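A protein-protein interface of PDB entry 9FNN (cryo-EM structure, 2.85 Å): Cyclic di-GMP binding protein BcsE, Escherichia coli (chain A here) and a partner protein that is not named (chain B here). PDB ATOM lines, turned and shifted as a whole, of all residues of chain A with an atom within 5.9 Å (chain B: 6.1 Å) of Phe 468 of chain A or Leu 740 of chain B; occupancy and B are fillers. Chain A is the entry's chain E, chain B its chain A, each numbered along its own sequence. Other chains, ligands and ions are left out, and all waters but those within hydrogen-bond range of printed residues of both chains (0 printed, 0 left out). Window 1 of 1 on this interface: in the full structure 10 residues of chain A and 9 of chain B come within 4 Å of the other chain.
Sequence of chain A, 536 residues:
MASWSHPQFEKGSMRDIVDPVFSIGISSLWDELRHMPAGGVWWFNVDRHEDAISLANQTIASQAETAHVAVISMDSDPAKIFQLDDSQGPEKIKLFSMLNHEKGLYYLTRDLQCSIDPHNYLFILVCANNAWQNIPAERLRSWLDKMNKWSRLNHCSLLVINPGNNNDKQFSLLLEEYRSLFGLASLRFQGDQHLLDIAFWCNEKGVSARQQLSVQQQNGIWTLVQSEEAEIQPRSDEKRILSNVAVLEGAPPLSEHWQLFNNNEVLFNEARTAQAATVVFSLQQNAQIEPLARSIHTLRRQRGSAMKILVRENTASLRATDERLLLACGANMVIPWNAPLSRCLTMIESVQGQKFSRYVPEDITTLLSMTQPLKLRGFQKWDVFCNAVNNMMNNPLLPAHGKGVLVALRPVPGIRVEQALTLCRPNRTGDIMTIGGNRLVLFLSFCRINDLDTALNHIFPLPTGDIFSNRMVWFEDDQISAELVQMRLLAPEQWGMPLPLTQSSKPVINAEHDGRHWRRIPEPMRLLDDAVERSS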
ATOM      1  N   LEU A 409     -30.384  34.195  22.164  1.00  0.00           N
ATOM      2  CA  LEU A 409     -29.931  32.812  22.154  1.00  0.00           C
ATOM      3  C   LEU A 409     -31.061  31.900  22.603  1.00  0.00           C
ATOM      4  O   LEU A 409     -31.645  32.107  23.671  1.00  0.00           O
ATOM      5  CB  LEU A 409     -28.714  32.622  23.063  1.00  0.00           C
ATOM      6  CG  LEU A 409     -27.367  33.237  22.674  1.00  0.00           C
ATOM      7  CD1 LEU A 409     -27.121  33.108  21.186  1.00  0.00           C
ATOM      8  CD2 LEU A 409     -27.266  34.686  23.120  1.00  0.00           C
ATOM      9  N   ARG A 410     -31.365  30.893  21.788  1.00  0.00           N
ATOM     10  CA  ARG A 410     -32.379  29.909  22.131  1.00  0.00           C
ATOM     11  C   ARG A 410     -31.698  28.645  22.625  1.00  0.00           C
ATOM     12  O   ARG A 410     -31.003  27.983  21.840  1.00  0.00           O
ATOM     13  CB  ARG A 410     -33.260  29.601  20.925  1.00  0.00           C
ATOM     14  CG  ARG A 410     -34.302  28.534  21.185  1.00  0.00           C
ATOM     15  CD  ARG A 410     -35.263  28.409  20.018  1.00  0.00           C
ATOM     16  NE  ARG A 410     -35.745  29.711  19.576  1.00  0.00           N
ATOM     17  CZ  ARG A 410     -36.681  30.418  20.194  1.00  0.00           C
ATOM     18  NH1 ARG A 410     -37.256  29.983  21.304  1.00  0.00           N
ATOM     19  NH2 ARG A 410     -37.049  31.590  19.688  1.00  0.00           N
ATOM     20  N   PRO A 411     -31.854  28.269  23.891  1.00  0.00           N
ATOM     21  CA  PRO A 411     -31.147  27.093  24.402  1.00  0.00           C
ATOM     22  C   PRO A 411     -31.633  25.810  23.752  1.00  0.00           C
ATOM     23  O   PRO A 411     -32.773  25.707  23.293  1.00  0.00           O
ATOM     24  CB  PRO A 411     -31.466  27.109  25.900  1.00  0.00           C
ATOM     25  CG  PRO A 411     -31.895  28.499  26.187  1.00  0.00           C
ATOM     26  CD  PRO A 411     -32.597  28.960  24.954  1.00  0.00           C
ATOM     27  N   VAL A 412     -30.741  24.826  23.711  1.00  0.00           N
ATOM     28  CA  VAL A 412     -31.070  23.499  23.203  1.00  0.00           C
ATOM     29  C   VAL A 412     -32.096  22.876  24.141  1.00  0.00           C
ATOM     30  O   VAL A 412     -32.131  23.222  25.331  1.00  0.00           O
ATOM     31  CB  VAL A 412     -29.819  22.615  23.078  1.00  0.00           C
ATOM     32  CG1 VAL A 412     -28.828  23.225  22.106  1.00  0.00           C
ATOM     33  CG2 VAL A 412     -29.174  22.408  24.434  1.00  0.00           C
ATOM     34  N   ILE A 415     -32.044  21.923  28.567  1.00  0.00           N
ATOM     35  CA  ILE A 415     -31.532  22.911  29.506  1.00  0.00           C
ATOM     36  C   ILE A 415     -32.414  24.148  29.435  1.00  0.00           C
ATOM     37  O   ILE A 415     -32.814  24.579  28.348  1.00  0.00           O
ATOM     38  CB  ILE A 415     -30.057  23.273  29.238  1.00  0.00           C
ATOM     39  CG1 ILE A 415     -29.864  23.778  27.810  1.00  0.00           C
ATOM     40  CG2 ILE A 415     -29.157  22.077  29.508  1.00  0.00           C
ATOM     41  CD1 ILE A 415     -28.449  24.206  27.520  1.00  0.00           C
ATOM     42  N   ALA A 420     -28.573  28.483  31.356  1.00  0.00           N
ATOM     43  CA  ALA A 420     -27.753  29.256  30.431  1.00  0.00           C
ATOM     44  C   ALA A 420     -27.315  30.569  31.061  1.00  0.00           C
ATOM     45  O   ALA A 420     -26.195  31.039  30.825  1.00  0.00           O
ATOM     46  CB  ALA A 420     -28.520  29.510  29.135  1.00  0.00           C
ATOM     47  N   LEU A 440     -32.354  33.755  25.853  1.00  0.00           N
ATOM     48  CA  LEU A 440     -31.348  34.518  26.576  1.00  0.00           C
ATOM     49  C   LEU A 440     -30.854  35.623  25.656  1.00  0.00           C
ATOM     50  O   LEU A 440     -30.319  35.345  24.578  1.00  0.00           O
ATOM     51  CB  LEU A 440     -30.195  33.625  27.031  1.00  0.00           C
ATOM     52  CG  LEU A 440     -29.169  34.253  27.973  1.00  0.00           C
ATOM     53  CD1 LEU A 440     -28.812  33.280  29.076  1.00  0.00           C
ATOM     54  CD2 LEU A 440     -27.929  34.665  27.215  1.00  0.00           C
ATOM     55  N   LEU A 456     -18.394  35.908  22.640  1.00  0.00           N
ATOM     56  CA  LEU A 456     -19.200  34.846  23.232  1.00  0.00           C
ATOM     57  C   LEU A 456     -18.321  33.763  23.845  1.00  0.00           C
ATOM     58  O   LEU A 456     -18.643  33.223  24.909  1.00  0.00           O
ATOM     59  CB  LEU A 456     -20.144  34.254  22.189  1.00  0.00           C
ATOM     60  CG  LEU A 456     -21.294  35.158  21.749  1.00  0.00           C
ATOM     61  CD1 LEU A 456     -22.280  34.391  20.898  1.00  0.00           C
ATOM     62  CD2 LEU A 456     -21.984  35.768  22.949  1.00  0.00           C
ATOM     63  N   PHE A 460     -18.845  32.581  27.666  1.00  0.00           N
ATOM     64  CA  PHE A 460     -19.393  31.314  28.127  1.00  0.00           C
ATOM     65  C   PHE A 460     -18.289  30.302  28.422  1.00  0.00           C
ATOM     66  O   PHE A 460     -17.243  30.302  27.768  1.00  0.00           O
ATOM     67  CB  PHE A 460     -20.351  30.736  27.081  1.00  0.00           C
ATOM     68  CG  PHE A 460     -21.532  31.618  26.792  1.00  0.00           C
ATOM     69  CD1 PHE A 460     -22.687  31.515  27.538  1.00  0.00           C
ATOM     70  CD2 PHE A 460     -21.488  32.547  25.772  1.00  0.00           C
ATOM     71  CE1 PHE A 460     -23.769  32.321  27.283  1.00  0.00           C
ATOM     72  CE2 PHE A 460     -22.571  33.355  25.510  1.00  0.00           C
ATOM     73  CZ  PHE A 460     -23.712  33.240  26.267  1.00  0.00           C
ATOM     74  N   THR A 464     -20.114  27.623  22.573  1.00  0.00           N
ATOM     75  CA  THR A 464     -21.412  28.119  22.136  1.00  0.00           C
ATOM     76  C   THR A 464     -21.829  27.322  20.908  1.00  0.00           C
ATOM     77  O   THR A 464     -21.219  27.446  19.842  1.00  0.00           O
ATOM     78  CB  THR A 464     -21.339  29.614  21.836  1.00  0.00           C
ATOM     79  OG1 THR A 464     -20.627  30.276  22.887  1.00  0.00           O
ATOM     80  CG2 THR A 464     -22.725  30.206  21.743  1.00  0.00           C
ATOM     81  N   GLY A 465     -22.866  26.506  21.056  1.00  0.00           N
ATOM     82  CA  GLY A 465     -23.245  25.568  20.021  1.00  0.00           C
ATOM     83  C   GLY A 465     -23.689  24.252  20.622  1.00  0.00           C
ATOM     84  O   GLY A 465     -24.533  23.550  20.057  1.00  0.00           O
ATOM     85  N   ASP A 466     -23.116  23.907  21.771  1.00  0.00           N
ATOM     86  CA  ASP A 466     -23.622  22.818  22.593  1.00  0.00           C
ATOM     87  C   ASP A 466     -24.611  23.296  23.642  1.00  0.00           C
ATOM     88  O   ASP A 466     -25.248  22.465  24.299  1.00  0.00           O
ATOM     89  CB  ASP A 466     -22.465  22.087  23.284  1.00  0.00           C
ATOM     90  CG  ASP A 466     -22.250  20.691  22.736  1.00  0.00           C
ATOM     91  OD1 ASP A 466     -23.202  20.123  22.160  1.00  0.00           O
ATOM     92  OD2 ASP A 466     -21.129  20.159  22.882  1.00  0.00           O
ATOM     93  N   ILE A 467     -24.753  24.609  23.808  1.00  0.00           N
ATOM     94  CA  ILE A 467     -25.694  25.170  24.759  1.00  0.00           C
ATOM     95  C   ILE A 467     -26.940  25.724  24.078  1.00  0.00           C
ATOM     96  O   ILE A 467     -28.030  25.660  24.659  1.00  0.00           O
ATOM     97  CB  ILE A 467     -25.014  26.261  25.614  1.00  0.00           C
ATOM     98  CG1 ILE A 467     -23.692  25.754  26.186  1.00  0.00           C
ATOM     99  CG2 ILE A 467     -25.921  26.704  26.747  1.00  0.00           C
ATOM    100  CD1 ILE A 467     -22.950  26.787  27.006  1.00  0.00           C
ATOM    101  N   PHE A 468     -26.822  26.250  22.861  1.00  0.00           N
ATOM    102  CA  PHE A 468     -27.923  26.923  22.191  1.00  0.00           C
ATOM    103  C   PHE A 468     -28.148  26.317  20.815  1.00  0.00           C
ATOM    104  O   PHE A 468     -27.222  25.799  20.185  1.00  0.00           O
ATOM    105  CB  PHE A 468     -27.654  28.423  22.069  1.00  0.00           C
ATOM    106  CG  PHE A 468     -27.214  29.058  23.353  1.00  0.00           C
ATOM    107  CD1 PHE A 468     -28.134  29.401  24.324  1.00  0.00           C
ATOM    108  CD2 PHE A 468     -25.877  29.307  23.593  1.00  0.00           C
ATOM    109  CE1 PHE A 468     -27.731  29.982  25.507  1.00  0.00           C
ATOM    110  CE2 PHE A 468     -25.469  29.886  24.775  1.00  0.00           C
ATOM    111  CZ  PHE A 468     -26.397  30.224  25.732  1.00  0.00           C
ATOM    112  N   SER A 469     -29.394  26.391  20.352  1.00  0.00           N
ATOM    113  CA  SER A 469     -29.795  25.818  19.074  1.00  0.00           C
ATOM    114  C   SER A 469     -29.803  26.832  17.941  1.00  0.00           C
ATOM    115  O   SER A 469     -29.415  26.498  16.819  1.00  0.00           O
ATOM    116  CB  SER A 469     -31.182  25.183  19.187  1.00  0.00           C
ATOM    117  OG  SER A 469     -31.157  24.047  20.031  1.00  0.00           O
ATOM    118  N   ASN A 470     -30.235  28.061  18.204  1.00  0.00           N
ATOM    119  CA  ASN A 470     -30.330  29.080  17.173  1.00  0.00           C
ATOM    120  C   ASN A 470     -29.865  30.412  17.739  1.00  0.00           C
ATOM    121  O   ASN A 470     -29.821  30.615  18.954  1.00  0.00           O
ATOM    122  CB  ASN A 470     -31.759  29.202  16.631  1.00  0.00           C
ATOM    123  CG  ASN A 470     -32.267  27.906  16.041  1.00  0.00           C
ATOM    124  OD1 ASN A 470     -32.104  27.645  14.850  1.00  0.00           O
ATOM    125  ND2 ASN A 470     -32.890  27.084  16.875  1.00  0.00           N
ATOM    126  N   ARG A 471     -29.510  31.322  16.838  1.00  0.00           N
ATOM    127  CA  ARG A 471     -28.994  32.626  17.222  1.00  0.00           C
ATOM    128  C   ARG A 471     -29.549  33.689  16.288  1.00  0.00           C
ATOM    129  O   ARG A 471     -29.519  33.520  15.066  1.00  0.00           O
ATOM    130  CB  ARG A 471     -27.462  32.633  17.190  1.00  0.00           C
ATOM    131  CG  ARG A 471     -26.837  33.923  17.658  1.00  0.00           C
ATOM    132  CD  ARG A 471     -25.354  33.752  17.914  1.00  0.00           C
ATOM    133  NE  ARG A 471     -24.579  33.714  16.683  1.00  0.00           N
ATOM    134  CZ  ARG A 471     -23.267  33.528  16.632  1.00  0.00           C
ATOM    135  NH1 ARG A 471     -22.556  33.330  17.728  1.00  0.00           N
ATOM    136  NH2 ARG A 471     -22.656  33.541  15.452  1.00  0.00           N
ATOM    137  N   GLN B 736     -27.764  17.876  14.917  1.00  0.00           N
ATOM    138  CA  GLN B 736     -27.386  19.286  15.022  1.00  0.00           C
ATOM    139  C   GLN B 736     -26.282  19.465  16.068  1.00  0.00           C
ATOM    140  O   GLN B 736     -26.469  20.063  17.131  1.00  0.00           O
ATOM    141  CB  GLN B 736     -28.602  20.163  15.338  1.00  0.00           C
ATOM    142  CG  GLN B 736     -28.329  21.657  15.243  1.00  0.00           C
ATOM    143  CD  GLN B 736     -29.511  22.494  15.683  1.00  0.00           C
ATOM    144  OE1 GLN B 736     -30.643  22.012  15.737  1.00  0.00           O
ATOM    145  NE2 GLN B 736     -29.254  23.756  16.008  1.00  0.00           N
ATOM    146  N   GLN B 738     -23.033  20.931  16.605  1.00  0.00           N
ATOM    147  CA  GLN B 738     -22.635  22.226  17.151  1.00  0.00           C
ATOM    148  C   GLN B 738     -22.471  23.201  15.995  1.00  0.00           C
ATOM    149  O   GLN B 738     -21.498  23.111  15.241  1.00  0.00           O
ATOM    150  CB  GLN B 738     -21.349  22.105  17.964  1.00  0.00           C
ATOM    151  CG  GLN B 738     -21.584  21.884  19.453  1.00  0.00           C
ATOM    152  CD  GLN B 738     -20.305  21.668  20.224  1.00  0.00           C
ATOM    153  OE1 GLN B 738     -19.538  20.751  19.935  1.00  0.00           O
ATOM    154  NE2 GLN B 738     -20.054  22.529  21.199  1.00  0.00           N
ATOM    155  N   ILE B 739     -23.413  24.130  15.866  1.00  0.00           N
ATOM    156  CA  ILE B 739     -23.363  25.149  14.826  1.00  0.00           C
ATOM    157  C   ILE B 739     -24.364  26.239  15.174  1.00  0.00           C
ATOM    158  O   ILE B 739     -25.462  25.952  15.665  1.00  0.00           O
ATOM    159  CB  ILE B 739     -23.654  24.548  13.436  1.00  0.00           C
ATOM    160  CG1 ILE B 739     -22.552  23.575  13.009  1.00  0.00           C
ATOM    161  CG2 ILE B 739     -23.854  25.648  12.388  1.00  0.00           C
ATOM    162  CD1 ILE B 739     -22.919  22.757  11.776  1.00  0.00           C
ATOM    163  N   LEU B 740     -24.003  27.492  14.905  1.00  0.00           N
ATOM    164  CA  LEU B 740     -24.891  28.629  15.094  1.00  0.00           C
ATOM    165  C   LEU B 740     -24.876  29.491  13.841  1.00  0.00           C
ATOM    166  O   LEU B 740     -23.990  29.376  12.994  1.00  0.00           O
ATOM    167  CB  LEU B 740     -24.505  29.460  16.321  1.00  0.00           C
ATOM    168  CG  LEU B 740     -24.902  28.867  17.670  1.00  0.00           C
ATOM    169  CD1 LEU B 740     -24.667  29.879  18.762  1.00  0.00           C
ATOM    170  CD2 LEU B 740     -26.349  28.424  17.648  1.00  0.00           C
ATOM    171  N   GLU B 741     -25.867  30.369  13.737  1.00  0.00           N
ATOM    172  CA  GLU B 741     -26.196  31.022  12.468  1.00  0.00           C
ATOM    173  C   GLU B 741     -25.200  32.077  12.032  1.00  0.00           C
ATOM    174  O   GLU B 741     -25.515  32.772  11.058  1.00  0.00           O
ATOM    175  CB  GLU B 741     -27.590  31.640  12.548  1.00  0.00           C
ATOM    176  CG  GLU B 741     -28.665  30.644  12.913  1.00  0.00           C
ATOM    177  CD  GLU B 741     -30.042  31.256  12.903  1.00  0.00           C
ATOM    178  OE1 GLU B 741     -30.167  32.422  12.474  1.00  0.00           O
ATOM    179  OE2 GLU B 741     -30.999  30.575  13.325  1.00  0.00           O
ATOM    180  N   GLY B 742     -24.044  32.271  12.655  1.00  0.00           N
ATOM    181  CA  GLY B 742     -23.071  33.203  12.123  1.00  0.00           C
ATOM    182  C   GLY B 742     -21.653  32.674  12.171  1.00  0.00           C
ATOM    183  O   GLY B 742     -20.723  33.321  11.683  1.00  0.00           O
ATOM    184  N   GLN B 743     -21.482  31.491  12.749  1.00  0.00           N
ATOM    185  CA  GLN B 743     -20.152  30.957  12.996  1.00  0.00           C
ATOM    186  C   GLN B 743     -19.453  30.589  11.695  1.00  0.00           C
ATOM    187  O   GLN B 743     -20.077  30.105  10.748  1.00  0.00           O
ATOM    188  CB  GLN B 743     -20.235  29.732  13.901  1.00  0.00           C
ATOM    189  CG  GLN B 743     -20.801  30.010  15.271  1.00  0.00           C
ATOM    190  CD  GLN B 743     -20.733  28.802  16.178  1.00  0.00           C
ATOM    191  OE1 GLN B 743     -21.380  28.759  17.223  1.00  0.00           O
ATOM    192  NE2 GLN B 743     -19.943  27.813  15.784  1.00  0.00           N
ATOM    193  N   VAL B 762     -22.083  29.956   8.365  1.00  0.00           N
ATOM    194  CA  VAL B 762     -23.417  29.394   8.515  1.00  0.00           C
ATOM    195  C   VAL B 762     -24.440  30.493   8.272  1.00  0.00           C
ATOM    196  O   VAL B 762     -24.337  31.587   8.836  1.00  0.00           O
ATOM    197  CB  VAL B 762     -23.586  28.764   9.906  1.00  0.00           C
ATOM    198  CG1 VAL B 762     -24.944  28.119  10.028  1.00  0.00           C
ATOM    199  CG2 VAL B 762     -22.485  27.751  10.176  1.00  0.00           C
ATOM    200  N   ALA B 763     -25.413  30.217   7.410  1.00  0.00           N
ATOM    201  CA  ALA B 763     -26.475  31.164   7.094  1.00  0.00           C
ATOM    202  C   ALA B 763     -27.811  30.795   7.713  1.00  0.00           C
ATOM    203  O   ALA B 763     -28.539  31.680   8.167  1.00  0.00           O
ATOM    204  CB  ALA B 763     -26.635  31.290   5.575  1.00  0.00           C
ATOM    205  N   VAL B 765     -29.857  27.606  10.200  1.00  0.00           N
ATOM    206  CA  VAL B 765     -29.890  26.381  10.997  1.00  0.00           C
ATOM    207  C   VAL B 765     -31.351  26.097  11.303  1.00  0.00           C
ATOM    208  O   VAL B 765     -32.009  26.886  11.994  1.00  0.00           O
ATOM    209  CB  VAL B 765     -29.087  26.494  12.296  1.00  0.00           C
ATOM    210  CG1 VAL B 765     -28.917  25.124  12.933  1.00  0.00           C
ATOM    211  CG2 VAL B 765     -27.759  27.141  12.042  1.00  0.00           C
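The backbone carbonyl oxygen (O) of Val 765 of chain B sits close to the side-chain amide oxygen (OD1) of Asn 470 of chain A, 3.0 Å away. NH2 of Arg 471 of chain A lies close to N of Gly 742 of chain B (3.4 Å). NE2 of Gln 736 of chain B is in hydrogen-bond range of O of Ser 469 of chain A, 2.9 Å away. NE2 of Gln 738 of chain B is in hydrogen-bond range of OD2 of Asp 466 of chain A (3.1 Å). The backbone carbonyl oxygen of Thr 464 of chain A lies close to the side-chain amide oxygen of Gln 743 of chain B, at 2.9 Å. OE2 of Glu 741 of chain B sits close to OD1 of Asn 470 of chain A, 3.5 Å away. The backbone carbonyl oxygen of Arg 471 of chain A sits close to the side-chain carboxylate of Glu 741 of chain B (2.9 Å).
The backbone NH of Arg 410 of chain A lies within hydrogen-bond range of the backbone carbonyl oxygen of Asn 470 of chain A (3.2 Å). The backbone carbonyl oxygen (O) of Arg 410 of chain A lies within hydrogen-bond range of the backbone NH (N) of Ser 469 of chain A, 2.7 Å away. The backbone carbonyl oxygen (O) of Gln 743 of chain B is in hydrogen-bond range of the backbone NH (N) of Val 762 of chain B (3.1 Å).
Among the printed residues, pairs that only touch across the chains: Gly 465 of chain A with Gln 738 of chain B (3.4 Å), Thr 464 of chain A with Leu 740 of chain B (3.6 Å), Arg 471 of chain A with Gln 743 of chain B (3.6 Å), Ser 469 of chain A with Leu 740 of chain B (3.7 Å), Phe 468 of chain A with Leu 740 of chain B (3.8 Å) and Asn 470 of chain A with Leu 740 of chain B (3.9 Å).
Phe 468 of chain A touches one residue of chain B. Of chain A, only Thr 464, Phe 468, Ser 469 and Asn 470 come within 4 Å of Leu 740 of chain B. Of the printed residues of chain A, Gln 738 of chain B touches Gly 465 and Asp 466. Of the printed residues of chain B, Asn 470 of chain A touches Leu 740, Glu 741 and Val 765. Printed residues of chain A within 4 Å of Gln 736 of chain B: Ser 469 (2.9 Å). Of the printed residues of chain A, Val 765 of chain B touches Asn 470. Leu 456 of chain A touches none of the printed residues of chain B. The nearest printed residue of chain A that does not touch Glu 741 of chain B is Ser 469 of chain A (5.6 Å).
Printed residues of chain B that touch a printed residue of chain A: Gln 736, Gln 738, Leu 740, Glu 741, Gly 742, Gln 743 and Val 765. Of the 17 printed residues of chain A, 7 touch a printed residue of chain B. Printed residues of chain A that touch a printed residue of chain B: Thr 464, Gly 465, Asp 466, Phe 468, Ser 469, Asn 470 and Arg 471. Among the printed residues, 13 pairs touch across the chains. Among the printed residues, no Asp or Glu carboxylate lies within 4 Å of a Lys or Arg side-chain nitrogen of the other chain.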
